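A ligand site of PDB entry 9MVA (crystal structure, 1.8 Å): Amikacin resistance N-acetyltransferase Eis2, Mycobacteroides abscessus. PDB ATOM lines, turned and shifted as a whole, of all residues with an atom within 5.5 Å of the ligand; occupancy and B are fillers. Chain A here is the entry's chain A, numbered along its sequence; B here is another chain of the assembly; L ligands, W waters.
OD1 of Asp 267 of chain B lies within salt-bridge range of NH2 of Arg 92. The side-chain carboxylate (OD2) of Asp 267 of chain B lies within salt-bridge range of the guanidinium group (NE) of Arg 91 (2.9 Å). The side-chain hydroxyl (OG1) of Thr 98 is in hydrogen-bond range of the backbone carbonyl oxygen (O) of Gly 94 (3.2 Å). NE of Arg 127 is in hydrogen-bond range of O of Ile 124, at 2.8 Å. The backbone carbonyl oxygen of Leu 123 is in hydrogen-bond range of the guanidinium group of Arg 127.
O of Phe 118 sits close to S1 of the ligand. Residues that only touch the ligand: Val 26 (3.4 Å), Phe 27 (3.6 Å), Val 81 (3.6 Å), Thr 82 (3.7 Å), Thr 85 (3.4 Å), Arg 91 (3.6 Å), Arg 93 (3.6 Å), Leu 95 (3.5 Å), Ala 119 (3.9 Å), Leu 123 (3.8 Å), Ile 124 (3.5 Å) and Leu 268 of chain B (3.8 Å). Hydrophobic or aromatic side chains within 4 Å of the ligand: Val 26, Phe 27, Val 81, Val 84, Val 86, Leu 95, Leu 96, Leu 123, Ile 124, Tyr 125 and Leu 268 of chain B. 25 residues have an atom within 4 Å of the ligand: Val 26, Phe 27, Val 81, Thr 82, Ala 83, Val 84, Thr 85, Val 86, Arg 91, Arg 92, Arg 93, Gly 94, Leu 95, Leu 96, Thr 97, Phe 118, Ala 119, Ser 120, Glu 121, Leu 123, Ile 124, Tyr 125, Arg 127, Asp 267 of chain B and Leu 268 of chain B. The nearest printed residue that does not touch the ligand is Leu 117 (4.1 Å).
N of Ser 120 sits close to S1 of the ligand (3.5 Å). OG of Ser 120 lies within hydrogen-bond range of O16 of the ligand (2.6 Å). The backbone NH of Val 84 lies within hydrogen-bond range of an oxygen (O17) of the ligand (2.9 Å). O of Val 84 is in hydrogen-bond range of N7 of the ligand (2.7 Å). The backbone NH of Thr 97 lies within hydrogen-bond range of an oxygen (O8) of the ligand, at 2.9 Å. An oxygen (O8) of the ligand is in hydrogen-bond range of the side-chain hydroxyl (OG1) of Thr 97, at 2.7 Å. An oxygen (O14) of the ligand lies within hydrogen-bond range of the side-chain carboxylate (OD2) of Asp 267 of chain B, at 2.7 Å. An oxygen (O12) of the ligand lies within hydrogen-bond range of the backbone NH of Arg 92, 2.8 Å away. The guanidinium group of Arg 92 is in salt-bridge range of an oxygen (O12) of the ligand (2.9 Å). O15 of the ligand is in hydrogen-bond range of N of Val 86 (2.9 Å). The backbone NH of Gly 94 sits at hydrogen-bond distance from an oxygen (O9) of the ligand (3.0 Å). OE2 of Glu 121 lies within hydrogen-bond range of N1 of the ligand (3.0 Å). The backbone NH (N) of Leu 96 sits at hydrogen-bond distance from an oxygen (O11) of the ligand. An oxygen (O1) of the ligand lies within hydrogen-bond range of the guanidinium group (NE) of Arg 127 (3.1 Å). A sulfur (S1) of the ligand sits close to the side-chain hydroxyl (OH) of Tyr 125, 3.2 Å away. The backbone NH (N) of Ala 83 lies within hydrogen-bond range of an oxygen (O17) of the ligand, at 3.2 Å.
Water W3 bridges O6 of the ligand and NH1 of Arg 127. Water W1 lies within hydrogen-bond range of N2 of the ligand (2.7 Å), OE1 of Glu 121 (2.8 Å) and NH2 of Arg 144 of chain B (2.9 Å). Water W2 bridges the side-chain carboxylate of Glu 121 (2.8 Å) and a nitrogen (N6) of the ligand (2.8 Å). Water W6 lies within hydrogen-bond range of NE of Arg 92 (2.8 Å) and O2 of the ligand (3.2 Å).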
ATOM      1  N   VAL A  26     -35.575  -3.550  -9.138  1.00  0.00           N
ATOM      2  CA  VAL A  26     -35.060  -3.140  -7.832  1.00  0.00           C
ATOM      3  C   VAL A  26     -34.064  -2.003  -7.984  1.00  0.00           C
ATOM      4  O   VAL A  26     -34.002  -1.097  -7.135  1.00  0.00           O
ATOM      5  CB  VAL A  26     -34.450  -4.342  -7.092  1.00  0.00           C
ATOM      6  CG1 VAL A  26     -33.826  -3.881  -5.765  1.00  0.00           C
ATOM      7  CG2 VAL A  26     -35.515  -5.398  -6.833  1.00  0.00           C
ATOM      8  N   PHE A  27     -33.295  -1.981  -9.068  1.00  0.00           N
ATOM      9  CA  PHE A  27     -32.443  -0.836  -9.364  1.00  0.00           C
ATOM     10  C   PHE A  27     -33.200   0.339  -9.971  1.00  0.00           C
ATOM     11  O   PHE A  27     -32.568   1.297 -10.425  1.00  0.00           O
ATOM     12  CB  PHE A  27     -31.294  -1.256 -10.283  1.00  0.00           C
ATOM     13  CG  PHE A  27     -30.147  -1.875  -9.560  1.00  0.00           C
ATOM     14  CD1 PHE A  27     -29.139  -1.082  -9.032  1.00  0.00           C
ATOM     15  CD2 PHE A  27     -30.075  -3.243  -9.380  1.00  0.00           C
ATOM     16  CE1 PHE A  27     -28.078  -1.652  -8.333  1.00  0.00           C
ATOM     17  CE2 PHE A  27     -29.019  -3.823  -8.699  1.00  0.00           C
ATOM     18  CZ  PHE A  27     -28.018  -3.025  -8.173  1.00  0.00           C
ATOM     19  N   VAL A  81     -19.311 -11.867  -8.674  1.00  0.00           N
ATOM     20  CA  VAL A  81     -20.666 -11.796  -8.128  1.00  0.00           C
ATOM     21  C   VAL A  81     -21.426 -10.653  -8.784  1.00  0.00           C
ATOM     22  O   VAL A  81     -20.865  -9.584  -9.073  1.00  0.00           O
ATOM     23  CB  VAL A  81     -20.599 -11.669  -6.603  1.00  0.00           C
ATOM     24  CG1 VAL A  81     -21.986 -11.476  -5.999  1.00  0.00           C
ATOM     25  CG2 VAL A  81     -19.944 -12.927  -6.000  1.00  0.00           C
ATOM     26  N   THR A  82     -22.725 -10.888  -9.045  1.00  0.00           N
ATOM     27  CA  THR A  82     -23.516 -10.009  -9.893  1.00  0.00           C
ATOM     28  C   THR A  82     -24.999 -10.158  -9.545  1.00  0.00           C
ATOM     29  O   THR A  82     -25.415 -11.116  -8.889  1.00  0.00           O
ATOM     30  CB  THR A  82     -23.279 -10.335 -11.375  1.00  0.00           C
ATOM     31  OG1 THR A  82     -23.773  -9.272 -12.189  1.00  0.00           O
ATOM     32  CG2 THR A  82     -23.973 -11.634 -11.763  1.00  0.00           C
ATOM     33  N   ALA A  83     -25.784  -9.171  -9.989  1.00  0.00           N
ATOM     34  CA  ALA A  83     -27.256  -9.249  -9.975  1.00  0.00           C
ATOM     35  C   ALA A  83     -27.814  -9.528  -8.571  1.00  0.00           C
ATOM     36  O   ALA A  83     -28.709 -10.346  -8.386  1.00  0.00           O
ATOM     37  CB  ALA A  83     -27.745 -10.307 -10.972  1.00  0.00           C
ATOM     38  N   VAL A  84     -27.290  -8.815  -7.583  1.00  0.00           N
ATOM     39  CA  VAL A  84     -27.721  -8.988  -6.190  1.00  0.00           C
ATOM     40  C   VAL A  84     -28.836  -7.977  -5.902  1.00  0.00           C
ATOM     41  O   VAL A  84     -28.590  -6.775  -5.887  1.00  0.00           O
ATOM     42  CB  VAL A  84     -26.554  -8.822  -5.218  1.00  0.00           C
ATOM     43  CG1 VAL A  84     -27.079  -8.798  -3.790  1.00  0.00           C
ATOM     44  CG2 VAL A  84     -25.532  -9.962  -5.399  1.00  0.00           C
ATOM     45  N   THR A  85     -30.056  -8.470  -5.681  1.00  0.00           N
ATOM     46  CA  THR A  85     -31.197  -7.600  -5.371  1.00  0.00           C
ATOM     47  C   THR A  85     -32.183  -8.341  -4.499  1.00  0.00           C
ATOM     48  O   THR A  85     -32.279  -9.569  -4.541  1.00  0.00           O
ATOM     49  CB  THR A  85     -31.984  -7.132  -6.607  1.00  0.00           C
ATOM     50  OG1 THR A  85     -32.722  -8.237  -7.139  1.00  0.00           O
ATOM     51  CG2 THR A  85     -31.076  -6.538  -7.708  1.00  0.00           C
ATOM     52  N   VAL A  86     -32.946  -7.571  -3.717  1.00  0.00           N
ATOM     53  CA  VAL A  86     -34.111  -8.087  -2.999  1.00  0.00           C
ATOM     54  C   VAL A  86     -35.230  -7.060  -3.168  1.00  0.00           C
ATOM     55  O   VAL A  86     -35.000  -5.862  -3.019  1.00  0.00           O
ATOM     56  CB  VAL A  86     -33.808  -8.352  -1.511  1.00  0.00           C
ATOM     57  CG1 VAL A  86     -35.088  -8.721  -0.751  1.00  0.00           C
ATOM     58  CG2 VAL A  86     -32.755  -9.474  -1.364  1.00  0.00           C
ATOM     59  N   SER A  87     -36.418  -7.535  -3.516  1.00  0.00           N
ATOM     60  CA  SER A  87     -37.544  -6.660  -3.801  1.00  0.00           C
ATOM     61  C   SER A  87     -37.878  -5.797  -2.586  1.00  0.00           C
ATOM     62  O   SER A  87     -37.735  -6.240  -1.436  1.00  0.00           O
ATOM     63  CB  SER A  87     -38.757  -7.486  -4.209  1.00  0.00           C
ATOM     64  OG  SER A  87     -39.949  -6.707  -4.190  1.00  0.00           O
ATOM     65  N   HIS A  90     -39.754  -7.355   0.281  1.00  0.00           N
ATOM     66  CA  HIS A  90     -39.172  -8.463   1.036  1.00  0.00           C
ATOM     67  C   HIS A  90     -37.835  -8.105   1.689  1.00  0.00           C
ATOM     68  O   HIS A  90     -37.180  -9.004   2.230  1.00  0.00           O
ATOM     69  CB  HIS A  90     -38.983  -9.688   0.134  1.00  0.00           C
ATOM     70  CG  HIS A  90     -40.268 -10.325  -0.290  1.00  0.00           C
ATOM     71  ND1 HIS A  90     -41.087  -9.771  -1.250  1.00  0.00           N
ATOM     72  CD2 HIS A  90     -40.881 -11.459   0.116  1.00  0.00           C
ATOM     73  CE1 HIS A  90     -42.151 -10.538  -1.416  1.00  0.00           C
ATOM     74  NE2 HIS A  90     -42.045 -11.568  -0.592  1.00  0.00           N
ATOM     75  N   ARG A  91     -37.426  -6.842   1.664  1.00  0.00           N
ATOM     76  CA  ARG A  91     -36.116  -6.445   2.156  1.00  0.00           C
ATOM     77  C   ARG A  91     -36.053  -6.518   3.685  1.00  0.00           C
ATOM     78  O   ARG A  91     -37.065  -6.445   4.388  1.00  0.00           O
ATOM     79  CB  ARG A  91     -35.795  -5.016   1.721  1.00  0.00           C
ATOM     80  CG  ARG A  91     -36.828  -4.011   2.227  1.00  0.00           C
ATOM     81  CD  ARG A  91     -36.612  -2.625   1.642  1.00  0.00           C
ATOM     82  NE  ARG A  91     -35.342  -2.031   2.079  1.00  0.00           N
ATOM     83  CZ  ARG A  91     -35.149  -1.480   3.264  1.00  0.00           C
ATOM     84  NH1 ARG A  91     -36.100  -1.452   4.182  1.00  0.00           N
ATOM     85  NH2 ARG A  91     -33.965  -0.940   3.546  1.00  0.00           N
ATOM     86  N   ARG A  92     -34.808  -6.618   4.178  1.00  0.00           N
ATOM     87  CA  ARG A  92     -34.496  -6.603   5.607  1.00  0.00           C
ATOM     88  C   ARG A  92     -35.226  -7.711   6.352  1.00  0.00           C
ATOM     89  O   ARG A  92     -35.689  -7.534   7.479  1.00  0.00           O
ATOM     90  CB  ARG A  92     -34.774  -5.233   6.225  1.00  0.00           C
ATOM     91  CG  ARG A  92     -33.986  -4.096   5.560  1.00  0.00           C
ATOM     92  CD  ARG A  92     -32.479  -4.347   5.591  1.00  0.00           C
ATOM     93  NE  ARG A  92     -31.734  -3.180   5.116  1.00  0.00           N
ATOM     94  CZ  ARG A  92     -31.522  -2.908   3.830  1.00  0.00           C
ATOM     95  NH1 ARG A  92     -31.923  -3.733   2.879  1.00  0.00           N
ATOM     96  NH2 ARG A  92     -30.910  -1.778   3.507  1.00  0.00           N
ATOM     97  N   ARG A  93     -35.318  -8.874   5.703  1.00  0.00           N
ATOM     98  CA  ARG A  93     -35.785 -10.103   6.310  1.00  0.00           C
ATOM     99  C   ARG A  93     -34.742 -11.212   6.201  1.00  0.00           C
ATOM    100  O   ARG A  93     -35.058 -12.376   6.448  1.00  0.00           O
ATOM    101  CB  ARG A  93     -37.106 -10.543   5.676  1.00  0.00           C
ATOM    102  CG  ARG A  93     -38.211  -9.526   5.850  1.00  0.00           C
ATOM    103  CD  ARG A  93     -39.425  -9.841   5.007  1.00  0.00           C
ATOM    104  NE  ARG A  93     -40.460  -8.846   5.204  1.00  0.00           N
ATOM    105  CZ  ARG A  93     -41.589  -8.760   4.508  1.00  0.00           C
ATOM    106  NH2 ARG A  93     -42.428  -7.764   4.751  1.00  0.00           N
ATOM    107  N   GLY A  94     -33.515 -10.871   5.813  1.00  0.00           N
ATOM    108  CA  GLY A  94     -32.439 -11.828   5.738  1.00  0.00           C
ATOM    109  C   GLY A  94     -32.329 -12.585   4.435  1.00  0.00           C
ATOM    110  O   GLY A  94     -31.562 -13.556   4.377  1.00  0.00           O
ATOM    111  N   LEU A  95     -33.048 -12.182   3.376  1.00  0.00           N
ATOM    112  CA  LEU A  95     -32.968 -12.927   2.121  1.00  0.00           C
ATOM    113  C   LEU A  95     -31.575 -12.843   1.504  1.00  0.00           C
ATOM    114  O   LEU A  95     -31.025 -13.858   1.058  1.00  0.00           O
ATOM    115  CB  LEU A  95     -34.026 -12.447   1.138  1.00  0.00           C
ATOM    116  CG  LEU A  95     -35.472 -12.761   1.502  1.00  0.00           C
ATOM    117  CD1 LEU A  95     -36.369 -12.515   0.283  1.00  0.00           C
ATOM    118  CD2 LEU A  95     -35.595 -14.202   1.978  1.00  0.00           C
ATOM    119  N   LEU A  96     -30.984 -11.642   1.470  1.00  0.00           N
ATOM    120  CA  LEU A  96     -29.608 -11.523   0.975  1.00  0.00           C
ATOM    121  C   LEU A  96     -28.662 -12.391   1.798  1.00  0.00           C
ATOM    122  O   LEU A  96     -27.826 -13.112   1.246  1.00  0.00           O
ATOM    123  CB  LEU A  96     -29.131 -10.069   1.031  1.00  0.00           C
ATOM    124  CG  LEU A  96     -27.639  -9.962   0.711  1.00  0.00           C
ATOM    125  CD1 LEU A  96     -27.374 -10.451  -0.712  1.00  0.00           C
ATOM    126  CD2 LEU A  96     -27.097  -8.528   0.907  1.00  0.00           C
ATOM    127  N   THR A  97     -28.783 -12.319   3.132  1.00  0.00           N
ATOM    128  CA  THR A  97     -27.936 -13.113   4.004  1.00  0.00           C
ATOM    129  C   THR A  97     -28.034 -14.596   3.656  1.00  0.00           C
ATOM    130  O   THR A  97     -27.009 -15.293   3.565  1.00  0.00           O
ATOM    131  CB  THR A  97     -28.316 -12.879   5.455  1.00  0.00           C
ATOM    132  OG1 THR A  97     -27.961 -11.532   5.825  1.00  0.00           O
ATOM    133  CG2 THR A  97     -27.592 -13.852   6.376  1.00  0.00           C
ATOM    134  N   THR A  98     -29.243 -15.091   3.411  1.00  0.00           N
ATOM    135  CA  THR A  98     -29.399 -16.492   3.044  1.00  0.00           C
ATOM    136  C   THR A  98     -28.770 -16.776   1.677  1.00  0.00           C
ATOM    137  O   THR A  98     -28.072 -17.783   1.504  1.00  0.00           O
ATOM    138  CB  THR A  98     -30.873 -16.873   3.065  1.00  0.00           C
ATOM    139  OG1 THR A  98     -31.372 -16.729   4.402  1.00  0.00           O
ATOM    140  CG2 THR A  98     -31.080 -18.313   2.606  1.00  0.00           C
ATOM    141  N   LEU A 117     -16.584  -8.466  -6.295  1.00  0.00           N
ATOM    142  CA  LEU A 117     -17.758  -7.728  -6.752  1.00  0.00           C
ATOM    143  C   LEU A 117     -17.504  -6.238  -6.672  1.00  0.00           C
ATOM    144  O   LEU A 117     -16.613  -5.773  -5.960  1.00  0.00           O
ATOM    145  CB  LEU A 117     -19.016  -8.104  -5.945  1.00  0.00           C
ATOM    146  CG  LEU A 117     -19.027  -8.030  -4.412  1.00  0.00           C
ATOM    147  CD1 LEU A 117     -19.175  -6.593  -3.888  1.00  0.00           C
ATOM    148  CD2 LEU A 117     -20.149  -8.914  -3.851  1.00  0.00           C
ATOM    149  N   PHE A 118     -18.279  -5.488  -7.456  1.00  0.00           N
ATOM    150  CA  PHE A 118     -18.504  -4.069  -7.239  1.00  0.00           C
ATOM    151  C   PHE A 118     -19.741  -3.912  -6.363  1.00  0.00           C
ATOM    152  O   PHE A 118     -20.645  -4.748  -6.395  1.00  0.00           O
ATOM    153  CB  PHE A 118     -18.741  -3.329  -8.565  1.00  0.00           C
ATOM    154  CG  PHE A 118     -17.593  -3.389  -9.546  1.00  0.00           C
ATOM    155  CD1 PHE A 118     -16.598  -2.415  -9.535  1.00  0.00           C
ATOM    156  CD2 PHE A 118     -17.550  -4.363 -10.536  1.00  0.00           C
ATOM    157  CE1 PHE A 118     -15.559  -2.445 -10.475  1.00  0.00           C
ATOM    158  CE2 PHE A 118     -16.521  -4.402 -11.472  1.00  0.00           C
ATOM    159  CZ  PHE A 118     -15.522  -3.446 -11.441  1.00  0.00           C
ATOM    160  N   ALA A 119     -19.789  -2.838  -5.561  1.00  0.00           N
ATOM    161  CA  ALA A 119     -20.892  -2.625  -4.635  1.00  0.00           C
ATOM    162  C   ALA A 119     -21.635  -1.327  -4.962  1.00  0.00           C
ATOM    163  O   ALA A 119     -21.016  -0.260  -5.035  1.00  0.00           O
ATOM    164  CB  ALA A 119     -20.405  -2.562  -3.183  1.00  0.00           C
ATOM    165  N   SER A 120     -22.949  -1.425  -5.126  1.00  0.00           N
ATOM    166  CA  SER A 120     -23.777  -0.225  -5.185  1.00  0.00           C
ATOM    167  C   SER A 120     -23.587   0.618  -3.930  1.00  0.00           C
ATOM    168  O   SER A 120     -23.539   1.850  -4.000  1.00  0.00           O
ATOM    169  CB  SER A 120     -25.240  -0.617  -5.331  1.00  0.00           C
ATOM    170  OG  SER A 120     -25.622  -1.366  -4.185  1.00  0.00           O
ATOM    171  N   GLU A 121     -23.509  -0.045  -2.770  1.00  0.00           N
ATOM    172  CA  GLU A 121     -23.262   0.600  -1.474  1.00  0.00           C
ATOM    173  C   GLU A 121     -22.264  -0.284  -0.735  1.00  0.00           C
ATOM    174  O   GLU A 121     -22.579  -1.427  -0.384  1.00  0.00           O
ATOM    175  CB  GLU A 121     -24.561   0.756  -0.673  1.00  0.00           C
ATOM    176  CG  GLU A 121     -25.686   1.423  -1.463  1.00  0.00           C
ATOM    177  CD  GLU A 121     -26.834   1.864  -0.573  1.00  0.00           C
ATOM    178  OE1 GLU A 121     -26.695   2.909   0.114  1.00  0.00           O
ATOM    179  OE2 GLU A 121     -27.886   1.169  -0.561  1.00  0.00           O
ATOM    180  N   LEU A 123     -20.977  -0.638   2.160  1.00  0.00           N
ATOM    181  CA  LEU A 123     -21.186  -1.194   3.498  1.00  0.00           C
ATOM    182  C   LEU A 123     -22.012  -2.465   3.501  1.00  0.00           C
ATOM    183  O   LEU A 123     -22.095  -3.115   4.543  1.00  0.00           O
ATOM    184  CB  LEU A 123     -21.841  -0.142   4.414  1.00  0.00           C
ATOM    185  CG  LEU A 123     -23.358   0.077   4.319  1.00  0.00           C
ATOM    186  CD1 LEU A 123     -23.780   1.059   5.400  1.00  0.00           C
ATOM    187  CD2 LEU A 123     -23.799   0.569   2.922  1.00  0.00           C
ATOM    188  N   ILE A 124     -22.622  -2.850   2.364  1.00  0.00           N
ATOM    189  CA  ILE A 124     -23.464  -4.044   2.335  1.00  0.00           C
ATOM    190  C   ILE A 124     -22.669  -5.299   2.708  1.00  0.00           C
ATOM    191  O   ILE A 124     -23.165  -6.147   3.462  1.00  0.00           O
ATOM    192  CB  ILE A 124     -24.130  -4.205   0.950  1.00  0.00           C
ATOM    193  CG1 ILE A 124     -25.111  -3.066   0.657  1.00  0.00           C
ATOM    194  CG2 ILE A 124     -24.822  -5.561   0.847  1.00  0.00           C
ATOM    195  CD1 ILE A 124     -25.561  -3.047  -0.806  1.00  0.00           C
ATOM    196  N   TYR A 125     -21.445  -5.444   2.192  1.00  0.00           N
ATOM    197  CA  TYR A 125     -20.859  -6.781   2.085  1.00  0.00           C
ATOM    198  C   TYR A 125     -19.817  -7.149   3.143  1.00  0.00           C
ATOM    199  O   TYR A 125     -19.506  -8.336   3.261  1.00  0.00           O
ATOM    200  CB  TYR A 125     -20.246  -6.983   0.699  1.00  0.00           C
ATOM    201  CG  TYR A 125     -21.279  -7.011  -0.389  1.00  0.00           C
ATOM    202  CD1 TYR A 125     -22.042  -8.148  -0.607  1.00  0.00           C
ATOM    203  CD2 TYR A 125     -21.526  -5.885  -1.192  1.00  0.00           C
ATOM    204  CE1 TYR A 125     -23.008  -8.189  -1.587  1.00  0.00           C
ATOM    205  CE2 TYR A 125     -22.495  -5.917  -2.183  1.00  0.00           C
ATOM    206  CZ  TYR A 125     -23.229  -7.072  -2.365  1.00  0.00           C
ATOM    207  OH  TYR A 125     -24.186  -7.133  -3.346  1.00  0.00           O
ATOM    208  N   ARG A 127     -20.087  -7.560   6.215  1.00  0.00           N
ATOM    209  CA  ARG A 127     -20.653  -8.515   7.158  1.00  0.00           C
ATOM    210  C   ARG A 127     -20.599  -9.947   6.639  1.00  0.00           C
ATOM    211  O   ARG A 127     -20.824 -10.885   7.416  1.00  0.00           O
ATOM    212  CB  ARG A 127     -22.099  -8.122   7.453  1.00  0.00           C
ATOM    213  CG  ARG A 127     -22.993  -8.207   6.235  1.00  0.00           C
ATOM    214  CD  ARG A 127     -24.281  -7.406   6.410  1.00  0.00           C
ATOM    215  NE  ARG A 127     -24.080  -5.987   6.119  1.00  0.00           N
ATOM    216  CZ  ARG A 127     -24.229  -5.010   7.010  1.00  0.00           C
ATOM    217  NH1 ARG A 127     -24.641  -5.261   8.243  1.00  0.00           N
ATOM    218  NH2 ARG A 127     -23.977  -3.757   6.646  1.00  0.00           N
ATOM    219  N   PHE A 128     -20.349 -10.137   5.344  1.00  0.00           N
ATOM    220  CA  PHE A 128     -20.229 -11.470   4.765  1.00  0.00           C
ATOM    221  C   PHE A 128     -18.778 -11.868   4.531  1.00  0.00           C
ATOM    222  O   PHE A 128     -18.529 -12.947   3.969  1.00  0.00           O
ATOM    223  CB  PHE A 128     -21.020 -11.561   3.461  1.00  0.00           C
ATOM    224  CG  PHE A 128     -22.445 -11.077   3.594  1.00  0.00           C
ATOM    225  CD1 PHE A 128     -23.320 -11.690   4.478  1.00  0.00           C
ATOM    226  CD2 PHE A 128     -22.897 -10.006   2.844  1.00  0.00           C
ATOM    227  CE1 PHE A 128     -24.633 -11.236   4.607  1.00  0.00           C
ATOM    228  CE2 PHE A 128     -24.193  -9.549   2.972  1.00  0.00           C
ATOM    229  CZ  PHE A 128     -25.060 -10.173   3.845  1.00  0.00           C
ATOM    230  N   ARG B 144     -34.109   9.765   4.412  1.00  0.00           N
ATOM    231  CA  ARG B 144     -33.448   9.376   5.659  1.00  0.00           C
ATOM    232  C   ARG B 144     -33.679  10.356   6.794  1.00  0.00           C
ATOM    233  O   ARG B 144     -33.266  10.067   7.927  1.00  0.00           O
ATOM    234  CB  ARG B 144     -31.955   9.165   5.440  1.00  0.00           C
ATOM    235  CG  ARG B 144     -31.776   8.007   4.495  1.00  0.00           C
ATOM    236  CD  ARG B 144     -30.349   7.578   4.248  1.00  0.00           C
ATOM    237  NE  ARG B 144     -30.433   6.258   3.648  1.00  0.00           N
ATOM    238  CZ  ARG B 144     -29.432   5.407   3.539  1.00  0.00           C
ATOM    239  NH1 ARG B 144     -28.207   5.724   3.930  1.00  0.00           N
ATOM    240  NH2 ARG B 144     -29.668   4.203   3.021  1.00  0.00           N
ATOM    241  N   ASP B 267     -34.660   1.015  -0.970  1.00  0.00           N
ATOM    242  CA  ASP B 267     -33.222   1.104  -1.158  1.00  0.00           C
ATOM    243  C   ASP B 267     -32.886   1.919  -2.407  1.00  0.00           C
ATOM    244  O   ASP B 267     -33.668   1.965  -3.369  1.00  0.00           O
ATOM    245  CB  ASP B 267     -32.607  -0.289  -1.255  1.00  0.00           C
ATOM    246  CG  ASP B 267     -32.755  -1.086   0.027  1.00  0.00           C
ATOM    247  OD1 ASP B 267     -32.333  -0.594   1.098  1.00  0.00           O
ATOM    248  OD2 ASP B 267     -33.321  -2.196  -0.027  1.00  0.00           O
ATOM    249  N   LEU B 268     -31.710   2.553  -2.376  1.00  0.00           N
ATOM    250  CA  LEU B 268     -31.141   3.443  -3.387  1.00  0.00           C
ATOM    251  C   LEU B 268     -31.823   4.815  -3.411  1.00  0.00           C
ATOM    252  O   LEU B 268     -31.294   5.747  -4.020  1.00  0.00           O
ATOM    253  CB  LEU B 268     -31.168   2.849  -4.802  1.00  0.00           C
ATOM    254  CG  LEU B 268     -30.574   1.442  -4.916  1.00  0.00           C
ATOM    255  CD1 LEU B 268     -30.710   0.895  -6.331  1.00  0.00           C
ATOM    256  CD2 LEU B 268     -29.118   1.450  -4.478  1.00  0.00           C
HETATM  257  N1  LIG L   1     -28.272  -1.263   1.124  1.00  0.00           N
HETATM  258  C1  LIG L   1     -27.930  -1.458   2.464  1.00  0.00           C
HETATM  259  N2  LIG L   1     -27.490  -0.396   3.215  1.00  0.00           N
HETATM  260  C2  LIG L   1     -27.164  -0.608   4.552  1.00  0.00           C
HETATM  261  N3  LIG L   1     -27.246  -1.770   5.230  1.00  0.00           N
HETATM  262  C3  LIG L   1     -27.686  -2.836   4.466  1.00  0.00           C
HETATM  263  C4  LIG L   1     -28.047  -2.734   3.096  1.00  0.00           C
HETATM  264  N4  LIG L   1     -28.456  -4.002   2.634  1.00  0.00           N
HETATM  265  C5  LIG L   1     -28.339  -4.836   3.699  1.00  0.00           C
HETATM  266  N5  LIG L   1     -27.853  -4.163   4.832  1.00  0.00           N
HETATM  267  C6  LIG L   1     -27.672  -4.787   6.188  1.00  0.00           C
HETATM  268  O1  LIG L   1     -27.194  -6.076   6.080  1.00  0.00           O
HETATM  269  C7  LIG L   1     -29.093  -4.952   6.882  1.00  0.00           C
HETATM  270  O2  LIG L   1     -29.421  -3.797   7.568  1.00  0.00           O
HETATM  271  C8  LIG L   1     -28.739  -6.040   7.955  1.00  0.00           C
HETATM  272  O3  LIG L   1     -28.030  -5.532   8.949  1.00  0.00           O
HETATM  273  P1  LIG L   1     -28.368  -6.048  10.660  1.00  0.00           P
HETATM  274  O4  LIG L   1     -27.572  -5.048  11.470  1.00  0.00           O
HETATM  275  O5  LIG L   1     -29.886  -5.928  10.737  1.00  0.00           O
HETATM  276  O6  LIG L   1     -27.797  -7.449  10.595  1.00  0.00           O
HETATM  277  C9  LIG L   1     -27.770  -6.921   7.114  1.00  0.00           C
HETATM  278  C10 LIG L   1     -28.511  -8.149   6.540  1.00  0.00           C
HETATM  279  O7  LIG L   1     -29.400  -7.646   5.618  1.00  0.00           O
HETATM  280  P2  LIG L   1     -30.428  -8.632   4.698  1.00  0.00           P
HETATM  281  O8  LIG L   1     -29.825  -9.996   4.592  1.00  0.00           O
HETATM  282  O9  LIG L   1     -31.805  -8.498   5.276  1.00  0.00           O
HETATM  283  O10 LIG L   1     -30.496  -7.898   3.205  1.00  0.00           O
HETATM  284  P3  LIG L   1     -31.762  -7.716   2.241  1.00  0.00           P
HETATM  285  O11 LIG L   1     -32.469  -9.011   1.955  1.00  0.00           O
HETATM  286  O12 LIG L   1     -32.553  -6.504   2.608  1.00  0.00           O
HETATM  287  O13 LIG L   1     -31.009  -7.264   0.709  1.00  0.00           O
HETATM  288  C11 LIG L   1     -29.926  -6.450   0.720  1.00  0.00           C
HETATM  289  C12 LIG L   1     -29.849  -5.715  -0.699  1.00  0.00           C
HETATM  290  C13 LIG L   1     -29.796  -6.799  -1.780  1.00  0.00           C
HETATM  291  C14 LIG L   1     -28.614  -4.821  -0.764  1.00  0.00           C
HETATM  292  C15 LIG L   1     -31.187  -4.902  -0.877  1.00  0.00           C
HETATM  293  O14 LIG L   1     -31.121  -3.791  -0.018  1.00  0.00           O
HETATM  294  C16 LIG L   1     -31.351  -4.309  -2.341  1.00  0.00           C
HETATM  295  O15 LIG L   1     -31.802  -4.976  -3.245  1.00  0.00           O
HETATM  296  N6  LIG L   1     -30.983  -2.926  -2.605  1.00  0.00           N
HETATM  297  C17 LIG L   1     -31.159  -2.291  -3.941  1.00  0.00           C
HETATM  298  C18 LIG L   1     -30.250  -2.904  -5.068  1.00  0.00           C
HETATM  299  C19 LIG L   1     -28.776  -3.145  -4.618  1.00  0.00           C
HETATM  300  O16 LIG L   1     -28.117  -2.212  -4.203  1.00  0.00           O
HETATM  301  N7  LIG L   1     -28.175  -4.444  -4.655  1.00  0.00           N
HETATM  302  C20 LIG L   1     -26.776  -4.679  -4.259  1.00  0.00           C
HETATM  303  C21 LIG L   1     -25.969  -4.308  -5.520  1.00  0.00           C
HETATM  304  S1  LIG L   1     -24.151  -4.657  -5.396  1.00  0.00           S
HETATM  305  C22 LIG L   1     -23.587  -5.159  -7.117  1.00  0.00           C
HETATM  306  C23 LIG L   1     -23.993  -6.631  -7.330  1.00  0.00           C
HETATM  307  O17 LIG L   1     -25.077  -6.911  -7.805  1.00  0.00           O
HETATM  308  C24 LIG L   1     -23.027  -7.735  -6.878  1.00  0.00           C
HETATM  309  O   HOH W   1     -27.615   2.240   2.625  1.00  0.00           O
HETATM  310  O   HOH W   2     -28.991  -1.145  -1.655  1.00  0.00           O
HETATM  311  O   HOH W   3     -25.466  -7.891   9.588  1.00  0.00           O
HETATM  312  O   HOH W   4     -32.058  -8.056   8.012  1.00  0.00           O
HETATM  313  O   HOH W   5     -26.463 -10.434   7.937  1.00  0.00           O
HETATM  314  O   HOH W   6     -31.275  -1.274   7.142  1.00  0.00           O
HETATM  315  O   HOH W   7     -34.707  -9.759   3.058  1.00  0.00           O
HETATM  316  O   HOH W   8     -26.627  -1.283   7.921  1.00  0.00           O
